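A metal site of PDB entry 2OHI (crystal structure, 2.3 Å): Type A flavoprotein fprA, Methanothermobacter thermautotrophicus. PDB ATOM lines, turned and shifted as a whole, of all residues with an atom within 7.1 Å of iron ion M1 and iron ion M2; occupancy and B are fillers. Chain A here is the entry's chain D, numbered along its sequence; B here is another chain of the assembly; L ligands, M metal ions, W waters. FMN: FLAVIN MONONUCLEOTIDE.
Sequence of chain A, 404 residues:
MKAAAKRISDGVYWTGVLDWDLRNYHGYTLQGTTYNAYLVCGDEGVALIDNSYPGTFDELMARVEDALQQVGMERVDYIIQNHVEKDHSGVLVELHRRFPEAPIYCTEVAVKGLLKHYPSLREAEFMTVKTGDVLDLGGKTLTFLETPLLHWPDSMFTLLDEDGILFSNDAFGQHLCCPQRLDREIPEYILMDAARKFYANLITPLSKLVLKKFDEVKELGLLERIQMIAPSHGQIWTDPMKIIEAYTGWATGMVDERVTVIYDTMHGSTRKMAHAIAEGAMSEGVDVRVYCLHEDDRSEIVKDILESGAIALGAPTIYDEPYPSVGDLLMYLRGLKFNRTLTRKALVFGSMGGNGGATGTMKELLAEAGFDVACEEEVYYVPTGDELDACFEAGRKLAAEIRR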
ATOM      1  N   TYR A  25     -19.948  20.778 -17.209  1.00  0.00           N
ATOM      2  CA  TYR A  25     -19.913  19.456 -16.635  1.00  0.00           C
ATOM      3  C   TYR A  25     -20.382  19.511 -15.175  1.00  0.00           C
ATOM      4  O   TYR A  25     -19.693  20.043 -14.297  1.00  0.00           O
ATOM      5  CB  TYR A  25     -18.513  18.841 -16.796  1.00  0.00           C
ATOM      6  CG  TYR A  25     -18.355  17.469 -16.175  1.00  0.00           C
ATOM      7  CD1 TYR A  25     -19.285  16.450 -16.425  1.00  0.00           C
ATOM      8  CD2 TYR A  25     -17.264  17.198 -15.338  1.00  0.00           C
ATOM      9  CE1 TYR A  25     -19.147  15.182 -15.840  1.00  0.00           C
ATOM     10  CE2 TYR A  25     -17.108  15.919 -14.745  1.00  0.00           C
ATOM     11  CZ  TYR A  25     -18.060  14.927 -15.006  1.00  0.00           C
ATOM     12  OH  TYR A  25     -17.915  13.680 -14.420  1.00  0.00           O
ATOM     13  N   HIS A  26     -21.580  18.967 -14.937  1.00  0.00           N
ATOM     14  CA  HIS A  26     -22.263  19.005 -13.621  1.00  0.00           C
ATOM     15  C   HIS A  26     -22.221  20.363 -12.911  1.00  0.00           C
ATOM     16  O   HIS A  26     -22.011  20.429 -11.695  1.00  0.00           O
ATOM     17  CB  HIS A  26     -21.848  17.820 -12.718  1.00  0.00           C
ATOM     18  CG  HIS A  26     -20.443  17.866 -12.200  1.00  0.00           C
ATOM     19  ND1 HIS A  26     -19.544  16.845 -12.444  1.00  0.00           N
ATOM     20  CD2 HIS A  26     -19.779  18.775 -11.437  1.00  0.00           C
ATOM     21  CE1 HIS A  26     -18.379  17.140 -11.866  1.00  0.00           C
ATOM     22  NE2 HIS A  26     -18.504  18.301 -11.257  1.00  0.00           N
ATOM     23  N   THR A  34     -10.521  16.467 -20.992  1.00  0.00           N
ATOM     24  CA  THR A  34     -10.073  15.177 -21.466  1.00  0.00           C
ATOM     25  C   THR A  34     -10.452  14.100 -20.464  1.00  0.00           C
ATOM     26  O   THR A  34     -10.697  14.358 -19.285  1.00  0.00           O
ATOM     27  CB  THR A  34      -8.536  15.131 -21.712  1.00  0.00           C
ATOM     28  OG1 THR A  34      -7.824  15.399 -20.484  1.00  0.00           O
ATOM     29  CG2 THR A  34      -8.099  16.115 -22.818  1.00  0.00           C
ATOM     30  N   TYR A  35     -10.513  12.873 -20.975  1.00  0.00           N
ATOM     31  CA  TYR A  35     -10.614  11.674 -20.141  1.00  0.00           C
ATOM     32  C   TYR A  35      -9.344  10.906 -20.397  1.00  0.00           C
ATOM     33  O   TYR A  35      -9.164  10.316 -21.461  1.00  0.00           O
ATOM     34  CB  TYR A  35     -11.870  10.893 -20.500  1.00  0.00           C
ATOM     35  CG  TYR A  35     -13.057  11.808 -20.647  1.00  0.00           C
ATOM     36  CD1 TYR A  35     -13.650  12.388 -19.520  1.00  0.00           C
ATOM     37  CD2 TYR A  35     -13.576  12.116 -21.903  1.00  0.00           C
ATOM     38  CE1 TYR A  35     -14.724  13.262 -19.652  1.00  0.00           C
ATOM     39  CE2 TYR A  35     -14.643  12.979 -22.040  1.00  0.00           C
ATOM     40  CZ  TYR A  35     -15.209  13.544 -20.906  1.00  0.00           C
ATOM     41  OH  TYR A  35     -16.267  14.398 -21.012  1.00  0.00           O
ATOM     42  N   HIS A  83     -11.538   4.671 -10.311  1.00  0.00           N
ATOM     43  CA  HIS A  83     -12.777   5.386  -9.930  1.00  0.00           C
ATOM     44  C   HIS A  83     -13.996   4.903 -10.729  1.00  0.00           C
ATOM     45  O   HIS A  83     -13.878   4.619 -11.929  1.00  0.00           O
ATOM     46  CB  HIS A  83     -12.590   6.863 -10.291  1.00  0.00           C
ATOM     47  CG  HIS A  83     -13.490   7.814  -9.577  1.00  0.00           C
ATOM     48  ND1 HIS A  83     -13.280   9.177  -9.571  1.00  0.00           N
ATOM     49  CD2 HIS A  83     -14.609   7.615  -8.830  1.00  0.00           C
ATOM     50  CE1 HIS A  83     -14.217   9.771  -8.856  1.00  0.00           C
ATOM     51  NE2 HIS A  83     -15.035   8.849  -8.397  1.00  0.00           N
ATOM     52  N   GLU A  85     -16.852   6.614 -11.381  1.00  0.00           N
ATOM     53  CA  GLU A  85     -17.599   7.663 -12.085  1.00  0.00           C
ATOM     54  C   GLU A  85     -17.608   7.425 -13.602  1.00  0.00           C
ATOM     55  O   GLU A  85     -16.625   6.914 -14.158  1.00  0.00           O
ATOM     56  CB  GLU A  85     -17.041   9.041 -11.754  1.00  0.00           C
ATOM     57  CG  GLU A  85     -18.057  10.162 -11.979  1.00  0.00           C
ATOM     58  CD  GLU A  85     -17.554  11.512 -11.510  1.00  0.00           C
ATOM     59  OE1 GLU A  85     -17.395  11.709 -10.296  1.00  0.00           O
ATOM     60  OE2 GLU A  85     -17.301  12.384 -12.368  1.00  0.00           O
ATOM     61  N   ASP A  87     -17.327   9.208 -16.293  1.00  0.00           N
ATOM     62  CA  ASP A  87     -16.352   9.845 -17.182  1.00  0.00           C
ATOM     63  C   ASP A  87     -15.072   9.027 -17.325  1.00  0.00           C
ATOM     64  O   ASP A  87     -14.276   9.263 -18.236  1.00  0.00           O
ATOM     65  CB  ASP A  87     -16.054  11.323 -16.818  1.00  0.00           C
ATOM     66  CG  ASP A  87     -15.893  11.576 -15.317  1.00  0.00           C
ATOM     67  OD1 ASP A  87     -16.380  10.740 -14.518  1.00  0.00           O
ATOM     68  OD2 ASP A  87     -15.306  12.628 -14.936  1.00  0.00           O
ATOM     69  N   HIS A  88     -14.907   8.042 -16.436  1.00  0.00           N
ATOM     70  CA  HIS A  88     -13.733   7.168 -16.406  1.00  0.00           C
ATOM     71  C   HIS A  88     -14.109   5.687 -16.422  1.00  0.00           C
ATOM     72  O   HIS A  88     -13.238   4.858 -16.619  1.00  0.00           O
ATOM     73  CB  HIS A  88     -12.860   7.470 -15.169  1.00  0.00           C
ATOM     74  CG  HIS A  88     -12.637   8.936 -14.939  1.00  0.00           C
ATOM     75  ND1 HIS A  88     -11.847   9.704 -15.769  1.00  0.00           N
ATOM     76  CD2 HIS A  88     -13.120   9.770 -13.988  1.00  0.00           C
ATOM     77  CE1 HIS A  88     -11.864  10.959 -15.335  1.00  0.00           C
ATOM     78  NE2 HIS A  88     -12.623  11.026 -14.257  1.00  0.00           N
ATOM     79  N   HIS A 151     -11.573  11.606  -4.810  1.00  0.00           N
ATOM     80  CA  HIS A 151     -12.652  12.424  -4.232  1.00  0.00           C
ATOM     81  C   HIS A 151     -13.895  11.602  -3.858  1.00  0.00           C
ATOM     82  O   HIS A 151     -14.855  12.148  -3.291  1.00  0.00           O
ATOM     83  CB  HIS A 151     -12.958  13.699  -5.046  1.00  0.00           C
ATOM     84  CG  HIS A 151     -13.688  13.451  -6.336  1.00  0.00           C
ATOM     85  ND1 HIS A 151     -15.015  13.770  -6.495  1.00  0.00           N
ATOM     86  CD2 HIS A 151     -13.264  12.942  -7.516  1.00  0.00           C
ATOM     87  CE1 HIS A 151     -15.390  13.468  -7.730  1.00  0.00           C
ATOM     88  NE2 HIS A 151     -14.347  12.961  -8.368  1.00  0.00           N
ATOM     89  N   TRP A 152     -13.855  10.303  -4.175  1.00  0.00           N
ATOM     90  CA  TRP A 152     -14.970   9.352  -3.949  1.00  0.00           C
ATOM     91  C   TRP A 152     -14.568   8.213  -2.975  1.00  0.00           C
ATOM     92  O   TRP A 152     -13.380   7.897  -2.857  1.00  0.00           O
ATOM     93  CB  TRP A 152     -15.454   8.778  -5.297  1.00  0.00           C
ATOM     94  CG  TRP A 152     -16.436   9.674  -6.052  1.00  0.00           C
ATOM     95  CD1 TRP A 152     -16.508  11.041  -6.003  1.00  0.00           C
ATOM     96  CD2 TRP A 152     -17.466   9.267  -6.988  1.00  0.00           C
ATOM     97  NE1 TRP A 152     -17.503  11.500  -6.823  1.00  0.00           N
ATOM     98  CE2 TRP A 152     -18.116  10.440  -7.434  1.00  0.00           C
ATOM     99  CE3 TRP A 152     -17.903   8.021  -7.483  1.00  0.00           C
ATOM    100  CZ2 TRP A 152     -19.189  10.404  -8.362  1.00  0.00           C
ATOM    101  CZ3 TRP A 152     -18.974   7.993  -8.406  1.00  0.00           C
ATOM    102  CH2 TRP A 152     -19.597   9.178  -8.829  1.00  0.00           C
ATOM    103  N   SER A 155     -12.334   5.549  -4.706  1.00  0.00           N
ATOM    104  CA  SER A 155     -11.128   6.000  -5.413  1.00  0.00           C
ATOM    105  C   SER A 155      -9.873   5.268  -4.965  1.00  0.00           C
ATOM    106  O   SER A 155      -9.761   4.871  -3.819  1.00  0.00           O
ATOM    107  CB  SER A 155     -10.885   7.485  -5.146  1.00  0.00           C
ATOM    108  OG  SER A 155     -12.064   8.234  -5.271  1.00  0.00           O
ATOM    109  N   ASN A 169      -5.937   9.431 -10.519  1.00  0.00           N
ATOM    110  CA  ASN A 169      -7.321   9.684 -10.956  1.00  0.00           C
ATOM    111  C   ASN A 169      -7.656  11.195 -11.001  1.00  0.00           C
ATOM    112  O   ASN A 169      -6.942  11.929 -11.652  1.00  0.00           O
ATOM    113  CB  ASN A 169      -8.361   8.842 -10.193  1.00  0.00           C
ATOM    114  CG  ASN A 169      -9.637   8.603 -11.034  1.00  0.00           C
ATOM    115  OD1 ASN A 169      -9.694   7.685 -11.867  1.00  0.00           O
ATOM    116  ND2 ASN A 169     -10.663   9.442 -10.819  1.00  0.00           N
ATOM    117  N   ASP A 170      -8.689  11.662 -10.303  1.00  0.00           N
ATOM    118  CA  ASP A 170      -9.070  13.081 -10.431  1.00  0.00           C
ATOM    119  C   ASP A 170      -8.087  14.043  -9.765  1.00  0.00           C
ATOM    120  O   ASP A 170      -7.968  15.175 -10.205  1.00  0.00           O
ATOM    121  CB  ASP A 170     -10.486  13.351  -9.923  1.00  0.00           C
ATOM    122  CG  ASP A 170     -11.542  12.875 -10.891  1.00  0.00           C
ATOM    123  OD1 ASP A 170     -11.445  13.182 -12.094  1.00  0.00           O
ATOM    124  OD2 ASP A 170     -12.482  12.185 -10.433  1.00  0.00           O
ATOM    125  N   HIS A 175      -9.453  20.679 -15.957  1.00  0.00           N
ATOM    126  CA  HIS A 175     -10.354  20.560 -17.094  1.00  0.00           C
ATOM    127  C   HIS A 175      -9.892  21.380 -18.288  1.00  0.00           C
ATOM    128  O   HIS A 175     -10.314  22.526 -18.450  1.00  0.00           O
ATOM    129  CB  HIS A 175     -11.798  20.918 -16.691  1.00  0.00           C
ATOM    130  CG  HIS A 175     -12.496  19.814 -15.970  1.00  0.00           C
ATOM    131  ND1 HIS A 175     -12.632  18.557 -16.509  1.00  0.00           N
ATOM    132  CD2 HIS A 175     -13.064  19.767 -14.744  1.00  0.00           C
ATOM    133  CE1 HIS A 175     -13.294  17.792 -15.659  1.00  0.00           C
ATOM    134  NE2 HIS A 175     -13.558  18.504 -14.584  1.00  0.00           N
ATOM    135  N   PHE A 198     -10.271  23.510 -10.518  1.00  0.00           N
ATOM    136  CA  PHE A 198     -10.520  22.111 -10.226  1.00  0.00           C
ATOM    137  C   PHE A 198     -10.411  21.931  -8.712  1.00  0.00           C
ATOM    138  O   PHE A 198     -11.344  21.425  -8.079  1.00  0.00           O
ATOM    139  CB  PHE A 198      -9.537  21.260 -11.010  1.00  0.00           C
ATOM    140  CG  PHE A 198      -9.861  19.783 -11.064  1.00  0.00           C
ATOM    141  CD1 PHE A 198     -10.311  19.195 -12.252  1.00  0.00           C
ATOM    142  CD2 PHE A 198      -9.651  18.961  -9.948  1.00  0.00           C
ATOM    143  CE1 PHE A 198     -10.560  17.817 -12.330  1.00  0.00           C
ATOM    144  CE2 PHE A 198      -9.899  17.586 -10.013  1.00  0.00           C
ATOM    145  CZ  PHE A 198     -10.368  17.006 -11.222  1.00  0.00           C
ATOM    146  N   LEU A 202     -13.604  20.920  -6.301  1.00  0.00           N
ATOM    147  CA  LEU A 202     -13.586  19.461  -6.191  1.00  0.00           C
ATOM    148  C   LEU A 202     -12.830  18.924  -4.985  1.00  0.00           C
ATOM    149  O   LEU A 202     -13.217  17.890  -4.423  1.00  0.00           O
ATOM    150  CB  LEU A 202     -13.091  18.838  -7.507  1.00  0.00           C
ATOM    151  CG  LEU A 202     -14.146  18.980  -8.633  1.00  0.00           C
ATOM    152  CD1 LEU A 202     -13.542  19.097 -10.034  1.00  0.00           C
ATOM    153  CD2 LEU A 202     -15.243  17.885  -8.544  1.00  0.00           C
ATOM    154  N   SER A 232      -6.485  12.056 -14.367  1.00  0.00           N
ATOM    155  CA  SER A 232      -7.548  11.577 -15.245  1.00  0.00           C
ATOM    156  C   SER A 232      -8.161  12.672 -16.124  1.00  0.00           C
ATOM    157  O   SER A 232      -8.917  12.388 -17.043  1.00  0.00           O
ATOM    158  CB  SER A 232      -8.617  10.889 -14.398  1.00  0.00           C
ATOM    159  OG  SER A 232      -9.115  11.804 -13.450  1.00  0.00           O
ATOM    160  N   HIS A 233      -7.844  13.935 -15.823  1.00  0.00           N
ATOM    161  CA  HIS A 233      -8.306  15.065 -16.648  1.00  0.00           C
ATOM    162  C   HIS A 233      -7.148  15.995 -16.927  1.00  0.00           C
ATOM    163  O   HIS A 233      -6.308  16.252 -16.034  1.00  0.00           O
ATOM    164  CB  HIS A 233      -9.411  15.845 -15.934  1.00  0.00           C
ATOM    165  CG  HIS A 233     -10.704  15.098 -15.790  1.00  0.00           C
ATOM    166  ND1 HIS A 233     -11.659  15.077 -16.775  1.00  0.00           N
ATOM    167  CD2 HIS A 233     -11.205  14.375 -14.767  1.00  0.00           C
ATOM    168  CE1 HIS A 233     -12.684  14.335 -16.382  1.00  0.00           C
ATOM    169  NE2 HIS A 233     -12.439  13.910 -15.151  1.00  0.00           N
ATOM    170  N   HIS B 267     -25.489  13.176 -13.625  1.00  0.00           N
ATOM    171  CA  HIS B 267     -25.228  12.013 -14.470  1.00  0.00           C
ATOM    172  C   HIS B 267     -26.493  11.313 -14.935  1.00  0.00           C
ATOM    173  O   HIS B 267     -26.416  10.301 -15.616  1.00  0.00           O
ATOM    174  CB  HIS B 267     -24.306  11.039 -13.733  1.00  0.00           C
ATOM    175  CG  HIS B 267     -22.979  11.624 -13.360  1.00  0.00           C
ATOM    176  ND1 HIS B 267     -22.071  12.069 -14.298  1.00  0.00           N
ATOM    177  CD2 HIS B 267     -22.403  11.836 -12.160  1.00  0.00           C
ATOM    178  CE1 HIS B 267     -20.993  12.539 -13.691  1.00  0.00           C
ATOM    179  NE2 HIS B 267     -21.173  12.410 -12.386  1.00  0.00           N
HETATM  180  N1  FMN L   1     -22.730  11.008  -2.924  1.00  0.00           N
HETATM  181  C2  FMN L   1     -22.948  10.945  -1.564  1.00  0.00           C
HETATM  182  O2  FMN L   1     -23.624  10.037  -1.111  1.00  0.00           O
HETATM  183  N3  FMN L   1     -22.404  11.896  -0.736  1.00  0.00           N
HETATM  184  C4  FMN L   1     -21.624  12.927  -1.231  1.00  0.00           C
HETATM  185  O4  FMN L   1     -21.001  13.615  -0.425  1.00  0.00           O
HETATM  186  C4A FMN L   1     -21.381  13.006  -2.612  1.00  0.00           C
HETATM  187  N5  FMN L   1     -20.612  14.014  -3.180  1.00  0.00           N
HETATM  188  C5A FMN L   1     -20.401  14.061  -4.550  1.00  0.00           C
HETATM  189  C6  FMN L   1     -19.622  15.070  -5.128  1.00  0.00           C
HETATM  190  C7  FMN L   1     -19.428  15.100  -6.521  1.00  0.00           C
HETATM  191  C7M FMN L   1     -18.533  16.143  -7.121  1.00  0.00           C
HETATM  192  C8  FMN L   1     -19.995  14.109  -7.329  1.00  0.00           C
HETATM  193  C8M FMN L   1     -19.975  14.203  -8.839  1.00  0.00           C
HETATM  194  C9  FMN L   1     -20.758  13.113  -6.742  1.00  0.00           C
HETATM  195  C9A FMN L   1     -20.967  13.075  -5.367  1.00  0.00           C
HETATM  196  N10 FMN L   1     -21.737  12.064  -4.813  1.00  0.00           N
HETATM  197  C10 FMN L   1     -21.944  12.030  -3.446  1.00  0.00           C
HETATM  198  C1' FMN L   1     -22.228  10.890  -5.610  1.00  0.00           C
HETATM  199  C2' FMN L   1     -23.486  11.311  -6.351  1.00  0.00           C
HETATM  200  O2' FMN L   1     -24.541  11.559  -5.467  1.00  0.00           O
HETATM  201  C3' FMN L   1     -23.805  10.205  -7.340  1.00  0.00           C
HETATM  202  O3' FMN L   1     -22.866  10.260  -8.403  1.00  0.00           O
HETATM  203  C4' FMN L   1     -25.237  10.295  -7.842  1.00  0.00           C
HETATM  204  O4' FMN L   1     -25.616   8.980  -8.182  1.00  0.00           O
HETATM  205  C5' FMN L   1     -25.351  11.168  -9.077  1.00  0.00           C
HETATM  206  O5' FMN L   1     -26.724  11.248  -9.379  1.00  0.00           O
HETATM  207  P   FMN L   1     -27.266  11.906 -10.729  1.00  0.00           P
HETATM  208  O1P FMN L   1     -27.065  10.886 -11.827  1.00  0.00           O
HETATM  209  O2P FMN L   1     -28.753  12.113 -10.592  1.00  0.00           O
HETATM  210  O3P FMN L   1     -26.578  13.197 -11.009  1.00  0.00           O
HETATM  211 FE    FE M   1     -13.271  12.859 -13.445  1.00  0.00          FE
HETATM  212 FE    FE M   2     -14.712  11.983 -10.091  1.00  0.00          FE
HETATM  213  O   HOH W   1     -15.738  15.010 -10.137  1.00  0.00           O
HETATM  214  O   HOH W   2     -14.541  15.122 -12.337  1.00  0.00           O
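N of His 267 of chain B is in hydrogen-bond range of O3P of the ligand (2.8 Å).
The indole nitrogen (NE1) of Trp 152 sits close to a ring nitrogen (ND1) of His 151.
N of His 151 lies within hydrogen-bond range of OG of Ser 155 (3.4 Å).
A ring nitrogen (ND1) of His 233 is in hydrogen-bond range of the backbone carbonyl oxygen (O) of Thr 34 (2.8 Å).
OD2 of Asp 170 lies close to ND1 of His 83 (3.2 Å).
N of Asp 170 lies within hydrogen-bond range of OG of Ser 232 (3.2 Å).
The side-chain amide nitrogen (ND2) of Asn 169 sits close to the side-chain carboxylate (OD2) of Asp 170 (3.3 Å).
ND1 of His 83 lies within hydrogen-bond range of ND2 of Asn 169, at 2.9 Å.
OE1 of Glu 85 lies close to NE1 of Trp 152, 3.5 Å away.
Residues that only touch iron ion M2: His 83 (2.6 Å).
Within 4 Å of iron ion M2: His 83, Glu 85, His 151 and Asp 170.
Iron ion M1 is bound by a ring nitrogen (NE2) of His 88, a ring nitrogen (NE2) of His 233, the side-chain carboxylate (OD1) of Asp 170 and the side-chain carboxylate (OD2) of Asp 87.
Iron ion M1 has four donor atoms within binding distance.
Slightly farther from iron ion M1 lies water W2 (2.8 Å).
Of the 19 residues printed, 4 come within 4 Å of iron ion M1.
The nearest printed residue that does not touch iron ion M1 is Glu 85 (4.2 Å).
NE2 of His 151 is bound to iron ion M2.
Iron ion M2 is bound by OD2 of Asp 170, at 2.3 Å.
Iron ion M2 has two donor atoms within binding distance.
Slightly farther from iron ion M2 lies OE1 of Glu 85 (2.7 Å).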
